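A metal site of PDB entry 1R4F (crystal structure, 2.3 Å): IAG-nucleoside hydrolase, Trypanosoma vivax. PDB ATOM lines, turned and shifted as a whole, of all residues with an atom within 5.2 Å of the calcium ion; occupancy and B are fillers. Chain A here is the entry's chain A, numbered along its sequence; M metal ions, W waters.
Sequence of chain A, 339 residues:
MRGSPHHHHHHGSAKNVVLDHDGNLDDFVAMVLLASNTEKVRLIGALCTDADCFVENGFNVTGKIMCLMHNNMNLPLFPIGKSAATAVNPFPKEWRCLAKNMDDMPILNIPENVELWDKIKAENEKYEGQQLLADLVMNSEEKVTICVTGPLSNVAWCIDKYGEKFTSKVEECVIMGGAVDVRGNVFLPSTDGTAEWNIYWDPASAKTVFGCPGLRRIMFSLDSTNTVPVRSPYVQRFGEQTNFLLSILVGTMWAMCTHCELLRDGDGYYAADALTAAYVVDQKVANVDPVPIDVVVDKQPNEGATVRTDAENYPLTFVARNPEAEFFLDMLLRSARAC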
ATOM      1  N   ASP A  22       9.036 -18.274 -14.992  1.00  0.00           N
ATOM      2  CA  ASP A  22       8.669 -16.908 -14.630  1.00  0.00           C
ATOM      3  C   ASP A  22       7.308 -16.766 -13.957  1.00  0.00           C
ATOM      4  O   ASP A  22       6.586 -15.786 -14.171  1.00  0.00           O
ATOM      5  CB  ASP A  22       8.759 -15.978 -15.859  1.00  0.00           C
ATOM      6  CG  ASP A  22       7.905 -16.424 -17.017  1.00  0.00           C
ATOM      7  OD1 ASP A  22       7.838 -15.674 -18.011  1.00  0.00           O
ATOM      8  OD2 ASP A  22       7.312 -17.528 -16.952  1.00  0.00           O
ATOM      9  N   ASN A  24       4.033 -18.111 -14.063  1.00  0.00           N
ATOM     10  CA  ASN A  24       2.700 -17.954 -14.634  1.00  0.00           C
ATOM     11  C   ASN A  24       1.906 -19.252 -14.455  1.00  0.00           C
ATOM     12  O   ASN A  24       2.440 -20.252 -13.967  1.00  0.00           O
ATOM     13  CB  ASN A  24       2.790 -17.637 -16.111  1.00  0.00           C
ATOM     14  CG  ASN A  24       2.163 -16.329 -16.451  1.00  0.00           C
ATOM     15  OD1 ASN A  24       2.859 -15.314 -16.555  1.00  0.00           O
ATOM     16  ND2 ASN A  24       0.841 -16.320 -16.601  1.00  0.00           N
ATOM     17  N   ASP A  26       0.786 -21.641 -16.632  1.00  0.00           N
ATOM     18  CA  ASP A  26       1.384 -22.804 -17.247  1.00  0.00           C
ATOM     19  C   ASP A  26       2.768 -23.139 -16.682  1.00  0.00           C
ATOM     20  O   ASP A  26       3.150 -24.303 -16.657  1.00  0.00           O
ATOM     21  CB  ASP A  26       1.374 -22.684 -18.786  1.00  0.00           C
ATOM     22  CG  ASP A  26       2.089 -21.452 -19.300  1.00  0.00           C
ATOM     23  OD1 ASP A  26       2.060 -20.408 -18.611  1.00  0.00           O
ATOM     24  OD2 ASP A  26       2.656 -21.525 -20.418  1.00  0.00           O
ATOM     25  N   ASP A  27       3.492 -22.144 -16.176  1.00  0.00           N
ATOM     26  CA  ASP A  27       4.792 -22.395 -15.558  1.00  0.00           C
ATOM     27  C   ASP A  27       4.605 -23.328 -14.353  1.00  0.00           C
ATOM     28  O   ASP A  27       5.399 -24.237 -14.117  1.00  0.00           O
ATOM     29  CB  ASP A  27       5.410 -21.096 -15.065  1.00  0.00           C
ATOM     30  CG  ASP A  27       5.781 -20.163 -16.176  1.00  0.00           C
ATOM     31  OD1 ASP A  27       6.897 -20.257 -16.699  1.00  0.00           O
ATOM     32  OD2 ASP A  27       4.939 -19.336 -16.553  1.00  0.00           O
ATOM     33  N   THR A 149      11.003 -22.160 -19.048  1.00  0.00           N
ATOM     34  CA  THR A 149       9.650 -21.796 -19.416  1.00  0.00           C
ATOM     35  C   THR A 149       9.425 -20.292 -19.319  1.00  0.00           C
ATOM     36  O   THR A 149       8.307 -19.808 -19.463  1.00  0.00           O
ATOM     37  CB  THR A 149       8.590 -22.564 -18.567  1.00  0.00           C
ATOM     38  OG1 THR A 149       8.830 -22.349 -17.173  1.00  0.00           O
ATOM     39  CG2 THR A 149       8.651 -24.047 -18.856  1.00  0.00           C
ATOM     40  N   GLY A 150      10.516 -19.571 -19.074  1.00  0.00           N
ATOM     41  CA  GLY A 150      10.485 -18.121 -19.003  1.00  0.00           C
ATOM     42  C   GLY A 150      11.531 -17.596 -19.978  1.00  0.00           C
ATOM     43  O   GLY A 150      11.914 -18.319 -20.890  1.00  0.00           O
ATOM     44  N   ASN A 198       8.640 -14.658 -24.558  1.00  0.00           N
ATOM     45  CA  ASN A 198       9.813 -15.091 -23.802  1.00  0.00           C
ATOM     46  C   ASN A 198      11.108 -14.615 -24.456  1.00  0.00           C
ATOM     47  O   ASN A 198      12.039 -14.181 -23.766  1.00  0.00           O
ATOM     48  CB  ASN A 198       9.837 -16.616 -23.620  1.00  0.00           C
ATOM     49  CG  ASN A 198       8.783 -17.104 -22.619  1.00  0.00           C
ATOM     50  OD1 ASN A 198       8.402 -16.384 -21.698  1.00  0.00           O
ATOM     51  ND2 ASN A 198       8.325 -18.334 -22.802  1.00  0.00           N
ATOM     52  N   ASP A 273       4.016 -23.987 -21.711  1.00  0.00           N
ATOM     53  CA  ASP A 273       4.987 -24.469 -20.729  1.00  0.00           C
ATOM     54  C   ASP A 273       4.696 -25.888 -20.258  1.00  0.00           C
ATOM     55  O   ASP A 273       5.611 -26.633 -19.944  1.00  0.00           O
ATOM     56  CB  ASP A 273       5.054 -23.515 -19.529  1.00  0.00           C
ATOM     57  CG  ASP A 273       5.413 -22.108 -19.927  1.00  0.00           C
ATOM     58  OD1 ASP A 273       5.893 -21.938 -21.050  1.00  0.00           O
ATOM     59  OD2 ASP A 273       5.221 -21.167 -19.108  1.00  0.00           O
HETATM   60 CA    CA M   1       6.249 -18.821 -18.704  1.00  0.00          CA
HETATM   61  O   HOH W   1       3.659 -18.448 -20.379  1.00  0.00           O
HETATM   62  O   HOH W   2       5.954 -19.223 -21.346  1.00  0.00           O
HETATM   63  O   HOH W   3       6.623 -16.756 -19.822  1.00  0.00           O
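Along chain A the residues within 4 Å of the calcium ion span positions 22 to 273.
Water W3 lies within hydrogen-bond range of OD1 of Asp 22 (2.4 Å) and OD1 of Asn 198 (2.6 Å). Water W2 bridges the side-chain carboxylate of Asp 273 (2.7 Å) and the side-chain amide nitrogen of Asn 198 (2.9 Å).
N of Asn 24 lies close to OD2 of Asp 27 (2.9 Å). The backbone NH (N) of Asp 273 sits close to the side-chain carboxylate (OD2) of Asp 26.
The calcium ion is bound by water W3, at 2.4 Å. The backbone carbonyl oxygen (O) of Thr 149 binds the calcium ion. The side-chain carboxylate (OD2) of Asp 22 is bound to the calcium ion. OD1 of Asp 27 binds the calcium ion (2.5 Å). The calcium ion is bound by OD2 of Asp 27 (2.6 Å). OD2 of Asp 273 binds the calcium ion (2.6 Å). Water W2 is bound to the calcium ion. The calcium ion has seven donor atoms within binding distance. Slightly farther from the calcium ion lies water W1 (3.1 Å).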
